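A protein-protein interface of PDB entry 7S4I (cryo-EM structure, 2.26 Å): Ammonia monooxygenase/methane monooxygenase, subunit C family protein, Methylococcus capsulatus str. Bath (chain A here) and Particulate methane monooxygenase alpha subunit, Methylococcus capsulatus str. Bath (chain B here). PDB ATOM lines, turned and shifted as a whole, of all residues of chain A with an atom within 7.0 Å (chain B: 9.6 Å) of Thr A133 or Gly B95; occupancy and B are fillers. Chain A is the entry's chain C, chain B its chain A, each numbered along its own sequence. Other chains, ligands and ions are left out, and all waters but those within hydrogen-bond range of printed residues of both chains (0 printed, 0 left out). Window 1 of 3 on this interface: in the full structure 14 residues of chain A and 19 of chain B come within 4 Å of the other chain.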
ATOM      1  N   TRP A  45      -9.747 -25.378  -5.892  1.00  0.00           N
ATOM      2  CA  TRP A  45     -11.039 -24.864  -5.475  1.00  0.00           C
ATOM      3  C   TRP A  45     -10.831 -24.089  -4.184  1.00  0.00           C
ATOM      4  O   TRP A  45      -9.760 -24.162  -3.575  1.00  0.00           O
ATOM      5  CB  TRP A  45     -12.024 -26.008  -5.246  1.00  0.00           C
ATOM      6  CG  TRP A  45     -11.804 -27.156  -6.168  1.00  0.00           C
ATOM      7  CD1 TRP A  45     -12.409 -27.377  -7.366  1.00  0.00           C
ATOM      8  CD2 TRP A  45     -10.894 -28.242  -5.971  1.00  0.00           C
ATOM      9  NE1 TRP A  45     -11.941 -28.540  -7.927  1.00  0.00           N
ATOM     10  CE2 TRP A  45     -11.007 -29.089  -7.089  1.00  0.00           C
ATOM     11  CE3 TRP A  45      -9.994 -28.581  -4.956  1.00  0.00           C
ATOM     12  CZ2 TRP A  45     -10.256 -30.251  -7.220  1.00  0.00           C
ATOM     13  CZ3 TRP A  45      -9.251 -29.734  -5.087  1.00  0.00           C
ATOM     14  CH2 TRP A  45      -9.386 -30.555  -6.209  1.00  0.00           C
ATOM     15  N   ASP A 127      -2.400 -28.364 -16.570  1.00  0.00           N
ATOM     16  CA  ASP A 127      -3.108 -27.235 -17.149  1.00  0.00           C
ATOM     17  C   ASP A 127      -4.235 -27.703 -18.049  1.00  0.00           C
ATOM     18  O   ASP A 127      -5.336 -27.135 -18.010  1.00  0.00           O
ATOM     19  CB  ASP A 127      -2.121 -26.366 -17.930  1.00  0.00           C
ATOM     20  CG  ASP A 127      -2.804 -25.340 -18.799  1.00  0.00           C
ATOM     21  OD1 ASP A 127      -3.226 -24.303 -18.255  1.00  0.00           O
ATOM     22  OD2 ASP A 127      -2.915 -25.565 -20.023  1.00  0.00           O
ATOM     23  N   GLY A 128      -3.978 -28.735 -18.844  1.00  0.00           N
ATOM     24  CA  GLY A 128      -5.026 -29.347 -19.637  1.00  0.00           C
ATOM     25  C   GLY A 128      -6.212 -29.821 -18.817  1.00  0.00           C
ATOM     26  O   GLY A 128      -7.355 -29.456 -19.111  1.00  0.00           O
ATOM     27  N   THR A 129      -5.957 -30.622 -17.780  1.00  0.00           N
ATOM     28  CA  THR A 129      -7.067 -31.147 -16.986  1.00  0.00           C
ATOM     29  C   THR A 129      -7.730 -30.073 -16.139  1.00  0.00           C
ATOM     30  O   THR A 129      -8.862 -30.263 -15.695  1.00  0.00           O
ATOM     31  CB  THR A 129      -6.631 -32.299 -16.074  1.00  0.00           C
ATOM     32  OG1 THR A 129      -7.663 -32.558 -15.113  1.00  0.00           O
ATOM     33  CG2 THR A 129      -5.377 -31.962 -15.333  1.00  0.00           C
ATOM     34  N   TRP A 130      -7.048 -28.966 -15.868  1.00  0.00           N
ATOM     35  CA  TRP A 130      -7.704 -27.863 -15.180  1.00  0.00           C
ATOM     36  C   TRP A 130      -8.649 -27.106 -16.111  1.00  0.00           C
ATOM     37  O   TRP A 130      -9.800 -26.831 -15.750  1.00  0.00           O
ATOM     38  CB  TRP A 130      -6.646 -26.927 -14.590  1.00  0.00           C
ATOM     39  CG  TRP A 130      -7.175 -25.654 -14.016  1.00  0.00           C
ATOM     40  CD1 TRP A 130      -7.302 -24.459 -14.655  1.00  0.00           C
ATOM     41  CD2 TRP A 130      -7.646 -25.447 -12.680  1.00  0.00           C
ATOM     42  NE1 TRP A 130      -7.821 -23.518 -13.801  1.00  0.00           N
ATOM     43  CE2 TRP A 130      -8.044 -24.101 -12.581  1.00  0.00           C
ATOM     44  CE3 TRP A 130      -7.774 -26.272 -11.559  1.00  0.00           C
ATOM     45  CZ2 TRP A 130      -8.557 -23.559 -11.407  1.00  0.00           C
ATOM     46  CZ3 TRP A 130      -8.281 -25.732 -10.393  1.00  0.00           C
ATOM     47  CH2 TRP A 130      -8.667 -24.389 -10.326  1.00  0.00           C
ATOM     48  N   HIS A 131      -8.189 -26.803 -17.327  1.00  0.00           N
ATOM     49  CA  HIS A 131      -8.982 -25.966 -18.221  1.00  0.00           C
ATOM     50  C   HIS A 131     -10.124 -26.745 -18.860  1.00  0.00           C
ATOM     51  O   HIS A 131     -11.173 -26.170 -19.174  1.00  0.00           O
ATOM     52  CB  HIS A 131      -8.090 -25.336 -19.285  1.00  0.00           C
ATOM     53  CG  HIS A 131      -7.174 -24.286 -18.745  1.00  0.00           C
ATOM     54  ND1 HIS A 131      -7.532 -23.451 -17.708  1.00  0.00           N
ATOM     55  CD2 HIS A 131      -5.918 -23.930 -19.099  1.00  0.00           C
ATOM     56  CE1 HIS A 131      -6.531 -22.631 -17.442  1.00  0.00           C
ATOM     57  NE2 HIS A 131      -5.540 -22.901 -18.271  1.00  0.00           N
ATOM     58  N   GLN A 132      -9.950 -28.051 -19.067  1.00  0.00           N
ATOM     59  CA  GLN A 132     -11.071 -28.807 -19.620  1.00  0.00           C
ATOM     60  C   GLN A 132     -12.199 -29.019 -18.621  1.00  0.00           C
ATOM     61  O   GLN A 132     -13.268 -29.488 -19.025  1.00  0.00           O
ATOM     62  CB  GLN A 132     -10.607 -30.163 -20.160  1.00  0.00           C
ATOM     63  CG  GLN A 132      -9.451 -30.095 -21.136  1.00  0.00           C
ATOM     64  CD  GLN A 132      -9.896 -30.234 -22.575  1.00  0.00           C
ATOM     65  OE1 GLN A 132     -10.564 -31.201 -22.942  1.00  0.00           O
ATOM     66  NE2 GLN A 132      -9.523 -29.267 -23.403  1.00  0.00           N
ATOM     67  N   THR A 133     -12.003 -28.696 -17.341  1.00  0.00           N
ATOM     68  CA  THR A 133     -13.035 -28.923 -16.338  1.00  0.00           C
ATOM     69  C   THR A 133     -13.482 -27.685 -15.580  1.00  0.00           C
ATOM     70  O   THR A 133     -14.503 -27.757 -14.888  1.00  0.00           O
ATOM     71  CB  THR A 133     -12.579 -29.976 -15.319  1.00  0.00           C
ATOM     72  OG1 THR A 133     -11.860 -29.341 -14.255  1.00  0.00           O
ATOM     73  CG2 THR A 133     -11.702 -30.998 -15.991  1.00  0.00           C
ATOM     74  N   ILE A 134     -12.771 -26.563 -15.666  1.00  0.00           N
ATOM     75  CA  ILE A 134     -13.347 -25.330 -15.142  1.00  0.00           C
ATOM     76  C   ILE A 134     -13.453 -24.320 -16.275  1.00  0.00           C
ATOM     77  O   ILE A 134     -12.886 -24.520 -17.354  1.00  0.00           O
ATOM     78  CB  ILE A 134     -12.539 -24.765 -13.955  1.00  0.00           C
ATOM     79  CG1 ILE A 134     -11.100 -24.431 -14.355  1.00  0.00           C
ATOM     80  CG2 ILE A 134     -12.554 -25.740 -12.787  1.00  0.00           C
ATOM     81  CD1 ILE A 134     -10.879 -22.985 -14.740  1.00  0.00           C
ATOM     82  N   VAL A 135     -14.181 -23.234 -16.041  1.00  0.00           N
ATOM     83  CA  VAL A 135     -14.256 -22.119 -16.977  1.00  0.00           C
ATOM     84  C   VAL A 135     -13.134 -21.168 -16.597  1.00  0.00           C
ATOM     85  O   VAL A 135     -13.154 -20.579 -15.509  1.00  0.00           O
ATOM     86  CB  VAL A 135     -15.617 -21.414 -16.939  1.00  0.00           C
ATOM     87  CG1 VAL A 135     -15.587 -20.168 -17.807  1.00  0.00           C
ATOM     88  CG2 VAL A 135     -16.711 -22.354 -17.401  1.00  0.00           C
ATOM     89  N   GLU A 209     -12.041 -25.024 -25.697  1.00  0.00           N
ATOM     90  CA  GLU A 209     -10.909 -25.444 -24.827  1.00  0.00           C
ATOM     91  C   GLU A 209      -9.964 -26.382 -25.585  1.00  0.00           C
ATOM     92  O   GLU A 209      -8.951 -26.766 -24.973  1.00  0.00           O
ATOM     93  CB  GLU A 209     -11.437 -26.152 -23.579  1.00  0.00           C
ATOM     94  CG  GLU A 209     -11.475 -25.264 -22.352  1.00  0.00           C
ATOM     95  CD  GLU A 209     -10.155 -24.613 -21.981  1.00  0.00           C
ATOM     96  OE1 GLU A 209      -9.095 -25.207 -22.262  1.00  0.00           O
ATOM     97  OE2 GLU A 209     -10.193 -23.518 -21.399  1.00  0.00           O
ATOM     98  N   HIS B  33     -18.563 -19.500 -11.749  1.00  0.00           N
ATOM     99  CA  HIS B  33     -17.383 -19.019 -11.036  1.00  0.00           C
ATOM    100  C   HIS B  33     -16.541 -18.477 -12.180  1.00  0.00           C
ATOM    101  O   HIS B  33     -15.585 -17.731 -11.914  1.00  0.00           O
ATOM    102  CB  HIS B  33     -16.620 -20.133 -10.280  1.00  0.00           C
ATOM    103  CG  HIS B  33     -16.914 -20.239  -8.814  1.00  0.00           C
ATOM    104  ND1 HIS B  33     -18.185 -20.030  -8.352  1.00  0.00           N
ATOM    105  CD2 HIS B  33     -16.157 -20.552  -7.719  1.00  0.00           C
ATOM    106  CE1 HIS B  33     -18.200 -20.153  -7.042  1.00  0.00           C
ATOM    107  NE2 HIS B  33     -16.999 -20.520  -6.634  1.00  0.00           N
ATOM    108  N   GLY B  34     -16.925 -18.848 -13.411  1.00  0.00           N
ATOM    109  CA  GLY B  34     -16.218 -18.386 -14.620  1.00  0.00           C
ATOM    110  C   GLY B  34     -16.844 -17.133 -15.206  1.00  0.00           C
ATOM    111  O   GLY B  34     -16.423 -16.733 -16.301  1.00  0.00           O
ATOM    112  N   ASN B  90     -24.867 -27.443 -20.763  1.00  0.00           N
ATOM    113  CA  ASN B  90     -23.835 -27.924 -19.863  1.00  0.00           C
ATOM    114  C   ASN B  90     -24.141 -27.497 -18.430  1.00  0.00           C
ATOM    115  O   ASN B  90     -25.109 -26.784 -18.154  1.00  0.00           O
ATOM    116  CB  ASN B  90     -22.465 -27.412 -20.312  1.00  0.00           C
ATOM    117  CG  ASN B  90     -21.350 -28.395 -20.022  1.00  0.00           C
ATOM    118  OD1 ASN B  90     -21.582 -29.469 -19.471  1.00  0.00           O
ATOM    119  ND2 ASN B  90     -20.132 -28.031 -20.397  1.00  0.00           N
ATOM    120  N   VAL B  91     -23.299 -27.947 -17.504  1.00  0.00           N
ATOM    121  CA  VAL B  91     -23.406 -27.594 -16.093  1.00  0.00           C
ATOM    122  C   VAL B  91     -22.081 -26.992 -15.652  1.00  0.00           C
ATOM    123  O   VAL B  91     -21.022 -27.598 -15.853  1.00  0.00           O
ATOM    124  CB  VAL B  91     -23.761 -28.813 -15.220  1.00  0.00           C
ATOM    125  CG1 VAL B  91     -23.989 -28.383 -13.784  1.00  0.00           C
ATOM    126  CG2 VAL B  91     -24.986 -29.523 -15.767  1.00  0.00           C
ATOM    127  N   GLY B  92     -22.137 -25.806 -15.053  1.00  0.00           N
ATOM    128  CA  GLY B  92     -20.946 -25.175 -14.525  1.00  0.00           C
ATOM    129  C   GLY B  92     -20.643 -25.648 -13.120  1.00  0.00           C
ATOM    130  O   GLY B  92     -21.408 -25.373 -12.191  1.00  0.00           O
ATOM    131  N   MET B  93     -19.535 -26.359 -12.949  1.00  0.00           N
ATOM    132  CA  MET B  93     -19.233 -27.006 -11.683  1.00  0.00           C
ATOM    133  C   MET B  93     -17.756 -27.364 -11.657  1.00  0.00           C
ATOM    134  O   MET B  93     -17.130 -27.513 -12.713  1.00  0.00           O
ATOM    135  CB  MET B  93     -20.108 -28.249 -11.492  1.00  0.00           C
ATOM    136  CG  MET B  93     -19.569 -29.496 -12.154  1.00  0.00           C
ATOM    137  SD  MET B  93     -20.837 -30.754 -12.365  1.00  0.00           S
ATOM    138  CE  MET B  93     -21.966 -30.276 -11.070  1.00  0.00           C
ATOM    139  N   PRO B  94     -17.165 -27.500 -10.465  1.00  0.00           N
ATOM    140  CA  PRO B  94     -15.734 -27.823 -10.380  1.00  0.00           C
ATOM    141  C   PRO B  94     -15.452 -29.307 -10.534  1.00  0.00           C
ATOM    142  O   PRO B  94     -15.157 -29.992  -9.550  1.00  0.00           O
ATOM    143  CB  PRO B  94     -15.342 -27.333  -8.977  1.00  0.00           C
ATOM    144  CG  PRO B  94     -16.552 -26.650  -8.415  1.00  0.00           C
ATOM    145  CD  PRO B  94     -17.731 -27.170  -9.150  1.00  0.00           C
ATOM    146  N   GLY B  95     -15.532 -29.817 -11.759  1.00  0.00           N
ATOM    147  CA  GLY B  95     -15.338 -31.226 -11.996  1.00  0.00           C
ATOM    148  C   GLY B  95     -16.555 -32.024 -11.582  1.00  0.00           C
ATOM    149  O   GLY B  95     -17.546 -31.474 -11.097  1.00  0.00           O
ATOM    150  N   PRO B  96     -16.495 -33.342 -11.732  1.00  0.00           N
ATOM    151  CA  PRO B  96     -17.687 -34.181 -11.511  1.00  0.00           C
ATOM    152  C   PRO B  96     -18.045 -34.335 -10.032  1.00  0.00           C
ATOM    153  O   PRO B  96     -18.120 -35.445  -9.498  1.00  0.00           O
ATOM    154  CB  PRO B  96     -17.280 -35.515 -12.152  1.00  0.00           C
ATOM    155  CG  PRO B  96     -15.881 -35.342 -12.671  1.00  0.00           C
ATOM    156  CD  PRO B  96     -15.304 -34.150 -12.016  1.00  0.00           C
ATOM    157  N   VAL B  97     -18.273 -33.206  -9.359  1.00  0.00           N
ATOM    158  CA  VAL B  97     -18.850 -33.263  -8.020  1.00  0.00           C
ATOM    159  C   VAL B  97     -20.307 -33.701  -8.076  1.00  0.00           C
ATOM    160  O   VAL B  97     -20.838 -34.208  -7.080  1.00  0.00           O
ATOM    161  CB  VAL B  97     -18.712 -31.913  -7.295  1.00  0.00           C
ATOM    162  CG1 VAL B  97     -17.251 -31.498  -7.226  1.00  0.00           C
ATOM    163  CG2 VAL B  97     -19.547 -30.843  -7.980  1.00  0.00           C
ATOM    164  N   PHE B  98     -20.961 -33.508  -9.218  1.00  0.00           N
ATOM    165  CA  PHE B  98     -22.231 -34.137  -9.547  1.00  0.00           C
ATOM    166  C   PHE B  98     -22.028 -34.860 -10.868  1.00  0.00           C
ATOM    167  O   PHE B  98     -21.130 -34.502 -11.636  1.00  0.00           O
ATOM    168  CB  PHE B  98     -23.364 -33.116  -9.702  1.00  0.00           C
ATOM    169  CG  PHE B  98     -23.800 -32.471  -8.419  1.00  0.00           C
ATOM    170  CD1 PHE B  98     -23.183 -31.319  -7.964  1.00  0.00           C
ATOM    171  CD2 PHE B  98     -24.844 -32.999  -7.683  1.00  0.00           C
ATOM    172  CE1 PHE B  98     -23.588 -30.716  -6.792  1.00  0.00           C
ATOM    173  CE2 PHE B  98     -25.253 -32.401  -6.511  1.00  0.00           C
ATOM    174  CZ  PHE B  98     -24.626 -31.256  -6.068  1.00  0.00           C
ATOM    175  N   ILE B  99     -22.846 -35.864 -11.137  1.00  0.00           N
ATOM    176  CA  ILE B  99     -22.907 -36.452 -12.468  1.00  0.00           C
ATOM    177  C   ILE B  99     -24.222 -36.042 -13.113  1.00  0.00           C
ATOM    178  O   ILE B  99     -25.269 -36.023 -12.457  1.00  0.00           O
ATOM    179  CB  ILE B  99     -22.756 -37.981 -12.418  1.00  0.00           C
ATOM    180  CG1 ILE B  99     -23.804 -38.613 -11.505  1.00  0.00           C
ATOM    181  CG2 ILE B  99     -21.349 -38.366 -11.984  1.00  0.00           C
ATOM    182  CD1 ILE B  99     -24.268 -39.966 -11.977  1.00  0.00           C
ATOM    183  N   ARG B 100     -24.163 -35.688 -14.391  1.00  0.00           N
ATOM    184  CA  ARG B 100     -25.361 -35.293 -15.126  1.00  0.00           C
ATOM    185  C   ARG B 100     -26.127 -36.550 -15.509  1.00  0.00           C
ATOM    186  O   ARG B 100     -25.781 -37.237 -16.472  1.00  0.00           O
ATOM    187  CB  ARG B 100     -24.987 -34.471 -16.354  1.00  0.00           C
ATOM    188  CG  ARG B 100     -26.177 -33.876 -17.083  1.00  0.00           C
ATOM    189  CD  ARG B 100     -25.762 -33.229 -18.394  1.00  0.00           C
ATOM    190  NE  ARG B 100     -24.429 -33.640 -18.812  1.00  0.00           N
ATOM    191  CZ  ARG B 100     -23.490 -32.810 -19.243  1.00  0.00           C
ATOM    192  NH1 ARG B 100     -23.708 -31.508 -19.334  1.00  0.00           N
ATOM    193  NH2 ARG B 100     -22.303 -33.297 -19.591  1.00  0.00           N
ATOM    194  N   LEU B 128     -29.123 -33.842 -11.666  1.00  0.00           N
ATOM    195  CA  LEU B 128     -27.776 -34.087 -11.176  1.00  0.00           C
ATOM    196  C   LEU B 128     -27.824 -35.063 -10.011  1.00  0.00           C
ATOM    197  O   LEU B 128     -28.735 -35.008  -9.182  1.00  0.00           O
ATOM    198  CB  LEU B 128     -27.103 -32.785 -10.734  1.00  0.00           C
ATOM    199  CG  LEU B 128     -26.992 -31.678 -11.781  1.00  0.00           C
ATOM    200  CD1 LEU B 128     -26.391 -30.428 -11.171  1.00  0.00           C
ATOM    201  CD2 LEU B 128     -26.168 -32.148 -12.966  1.00  0.00           C
ATOM    202  N   LYS B 129     -26.841 -35.954  -9.953  1.00  0.00           N
ATOM    203  CA  LYS B 129     -26.692 -36.899  -8.856  1.00  0.00           C
ATOM    204  C   LYS B 129     -25.411 -36.576  -8.100  1.00  0.00           C
ATOM    205  O   LYS B 129     -24.339 -36.478  -8.705  1.00  0.00           O
ATOM    206  CB  LYS B 129     -26.665 -38.340  -9.369  1.00  0.00           C
ATOM    207  CG  LYS B 129     -26.656 -39.392  -8.276  1.00  0.00           C
ATOM    208  CD  LYS B 129     -26.279 -40.757  -8.826  1.00  0.00           C
ATOM    209  CE  LYS B 129     -27.260 -41.824  -8.378  1.00  0.00           C
ATOM    210  NZ  LYS B 129     -26.647 -43.178  -8.379  1.00  0.00           N
ATOM    211  N   ALA B 130     -25.527 -36.411  -6.785  1.00  0.00           N
ATOM    212  CA  ALA B 130     -24.387 -35.997  -5.979  1.00  0.00           C
ATOM    213  C   ALA B 130     -23.326 -37.089  -5.933  1.00  0.00           C
ATOM    214  O   ALA B 130     -23.633 -38.273  -5.770  1.00  0.00           O
ATOM    215  CB  ALA B 130     -24.840 -35.644  -4.566  1.00  0.00           C
ATOM    216  N   ARG B 131     -22.075 -36.682  -6.073  1.00  0.00           N
ATOM    217  CA  ARG B 131     -20.954 -37.612  -6.135  1.00  0.00           C
ATOM    218  C   ARG B 131     -19.847 -37.288  -5.145  1.00  0.00           C
ATOM    219  O   ARG B 131     -19.249 -38.207  -4.582  1.00  0.00           O
ATOM    220  CB  ARG B 131     -20.390 -37.632  -7.564  1.00  0.00           C
ATOM    221  CG  ARG B 131     -19.284 -38.644  -7.791  1.00  0.00           C
ATOM    222  CD  ARG B 131     -18.891 -38.690  -9.255  1.00  0.00           C
ATOM    223  NE  ARG B 131     -17.719 -39.525  -9.486  1.00  0.00           N
ATOM    224  CZ  ARG B 131     -16.497 -39.057  -9.697  1.00  0.00           C
ATOM    225  NH1 ARG B 131     -16.247 -37.758  -9.702  1.00  0.00           N
ATOM    226  NH2 ARG B 131     -15.503 -39.913  -9.908  1.00  0.00           N
ATOM    227  N   ARG B 132     -19.565 -36.009  -4.909  1.00  0.00           N
ATOM    228  CA  ARG B 132     -18.452 -35.601  -4.074  1.00  0.00           C
ATOM    229  C   ARG B 132     -18.933 -34.666  -2.973  1.00  0.00           C
ATOM    230  O   ARG B 132     -19.616 -33.674  -3.264  1.00  0.00           O
ATOM    231  CB  ARG B 132     -17.372 -34.904  -4.914  1.00  0.00           C
ATOM    232  CG  ARG B 132     -16.290 -35.835  -5.428  1.00  0.00           C
ATOM    233  CD  ARG B 132     -15.150 -35.051  -6.048  1.00  0.00           C
ATOM    234  NE  ARG B 132     -14.306 -34.435  -5.032  1.00  0.00           N
ATOM    235  CZ  ARG B 132     -13.709 -33.260  -5.167  1.00  0.00           C
ATOM    236  NH1 ARG B 132     -13.834 -32.545  -6.272  1.00  0.00           N
ATOM    237  NH2 ARG B 132     -12.970 -32.789  -4.167  1.00  0.00           N
ATOM    238  N   TRP B 136     -20.678 -26.706  -3.347  1.00  0.00           N
ATOM    239  CA  TRP B 136     -20.384 -26.489  -4.753  1.00  0.00           C
ATOM    240  C   TRP B 136     -21.310 -25.432  -5.336  1.00  0.00           C
ATOM    241  O   TRP B 136     -22.509 -25.397  -5.043  1.00  0.00           O
ATOM    242  CB  TRP B 136     -20.515 -27.791  -5.544  1.00  0.00           C
ATOM    243  CG  TRP B 136     -19.805 -28.940  -4.905  1.00  0.00           C
ATOM    244  CD1 TRP B 136     -20.371 -30.059  -4.373  1.00  0.00           C
ATOM    245  CD2 TRP B 136     -18.391 -29.077  -4.717  1.00  0.00           C
ATOM    246  NE1 TRP B 136     -19.401 -30.889  -3.872  1.00  0.00           N
ATOM    247  CE2 TRP B 136     -18.176 -30.308  -4.069  1.00  0.00           C
ATOM    248  CE3 TRP B 136     -17.289 -28.281  -5.035  1.00  0.00           C
ATOM    249  CZ2 TRP B 136     -16.903 -30.762  -3.737  1.00  0.00           C
ATOM    250  CZ3 TRP B 136     -16.027 -28.733  -4.703  1.00  0.00           C
ATOM    251  CH2 TRP B 136     -15.844 -29.962  -4.061  1.00  0.00           C
ATOM    252  N   HIS B 137     -20.738 -24.572  -6.169  1.00  0.00           N
ATOM    253  CA  HIS B 137     -21.480 -23.526  -6.864  1.00  0.00           C
ATOM    254  C   HIS B 137     -21.874 -24.080  -8.227  1.00  0.00           C
ATOM    255  O   HIS B 137     -21.047 -24.165  -9.138  1.00  0.00           O
ATOM    256  CB  HIS B 137     -20.642 -22.258  -6.982  1.00  0.00           C
ATOM    257  CG  HIS B 137     -21.453 -21.001  -7.008  1.00  0.00           C
ATOM    258  ND1 HIS B 137     -21.202 -19.971  -7.888  1.00  0.00           N
ATOM    259  CD2 HIS B 137     -22.513 -20.609  -6.262  1.00  0.00           C
ATOM    260  CE1 HIS B 137     -22.071 -18.998  -7.683  1.00  0.00           C
ATOM    261  NE2 HIS B 137     -22.878 -19.360  -6.703  1.00  0.00           N
ATOM    262  N   VAL B 138     -23.139 -24.456  -8.365  1.00  0.00           N
ATOM    263  CA  VAL B 138     -23.622 -25.134  -9.561  1.00  0.00           C
ATOM    264  C   VAL B 138     -24.279 -24.119 -10.484  1.00  0.00           C
ATOM    265  O   VAL B 138     -25.256 -23.461 -10.108  1.00  0.00           O
ATOM    266  CB  VAL B 138     -24.603 -26.260  -9.196  1.00  0.00           C
ATOM    267  CG1 VAL B 138     -24.964 -27.063 -10.430  1.00  0.00           C
ATOM    268  CG2 VAL B 138     -23.999 -27.156  -8.130  1.00  0.00           C
ATOM    269  N   MET B 141     -25.352 -23.677 -17.715  1.00  0.00           N
ATOM    270  CA  MET B 141     -24.668 -22.926 -18.751  1.00  0.00           C
ATOM    271  C   MET B 141     -25.000 -23.470 -20.135  1.00  0.00           C
ATOM    272  O   MET B 141     -25.402 -24.621 -20.307  1.00  0.00           O
ATOM    273  CB  MET B 141     -23.160 -22.955 -18.515  1.00  0.00           C
ATOM    274  CG  MET B 141     -22.612 -24.341 -18.261  1.00  0.00           C
ATOM    275  SD  MET B 141     -20.829 -24.351 -18.034  1.00  0.00           S
ATOM    276  CE  MET B 141     -20.320 -23.246 -19.343  1.00  0.00           C
ATOM    277  N   MET B 163     -17.573 -40.004  -0.814  1.00  0.00           N
ATOM    278  CA  MET B 163     -17.443 -40.349  -2.225  1.00  0.00           C
ATOM    279  C   MET B 163     -17.432 -41.856  -2.437  1.00  0.00           C
ATOM    280  O   MET B 163     -17.849 -42.334  -3.498  1.00  0.00           O
ATOM    281  CB  MET B 163     -16.175 -39.727  -2.804  1.00  0.00           C
ATOM    282  CG  MET B 163     -16.170 -39.654  -4.316  1.00  0.00           C
ATOM    283  SD  MET B 163     -14.615 -39.032  -4.968  1.00  0.00           S
ATOM    284  CE  MET B 163     -14.816 -39.430  -6.697  1.00  0.00           C
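O of Thr A129 sits close to OG1 of Thr A133, 3.5 Å away.
Of the 23 printed residues of chain B, 4 touch a printed residue of chain A.
Printed residues of chain B that touch a printed residue of chain A: Gly B34, Met B93, Pro B94 and Gly B95.
Hydrophobic or aromatic side chains of chain B within 4 Å of the printed part of chain A: Pro B94.
Among the printed residues, 4 pairs touch across the chains.
O of Thr A133 sits close to O of Met B93 (3.4 Å).
Among the printed residues, pairs that only touch across the chains: Trp A45 with Pro B94 (3.3 Å), Val A135 with Gly B34 (3.7 Å) and Thr A133 with Gly B95 (3.9 Å).
Of the printed residues of chain B, Trp A45 touches Pro B94 (3.3 Å).
Of chain B, only Met B93 and Gly B95 come within 4 Å of Thr A133.
Ile A134 touches none of the printed residues of chain B.
Printed residues of chain B within 4 Å of Val A135: Gly B34 (3.7 Å).
Of the printed residues of chain A, Gly B34 touches Val A135 (3.7 Å).
Printed residues of chain A within 4 Å of Met B93: Thr A133 (3.4 Å).
Printed residues of chain A within 4 Å of Pro B94: Trp A45.
The nearest printed residue of chain B that does not touch Val A135 is Met B141 (4.2 Å).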
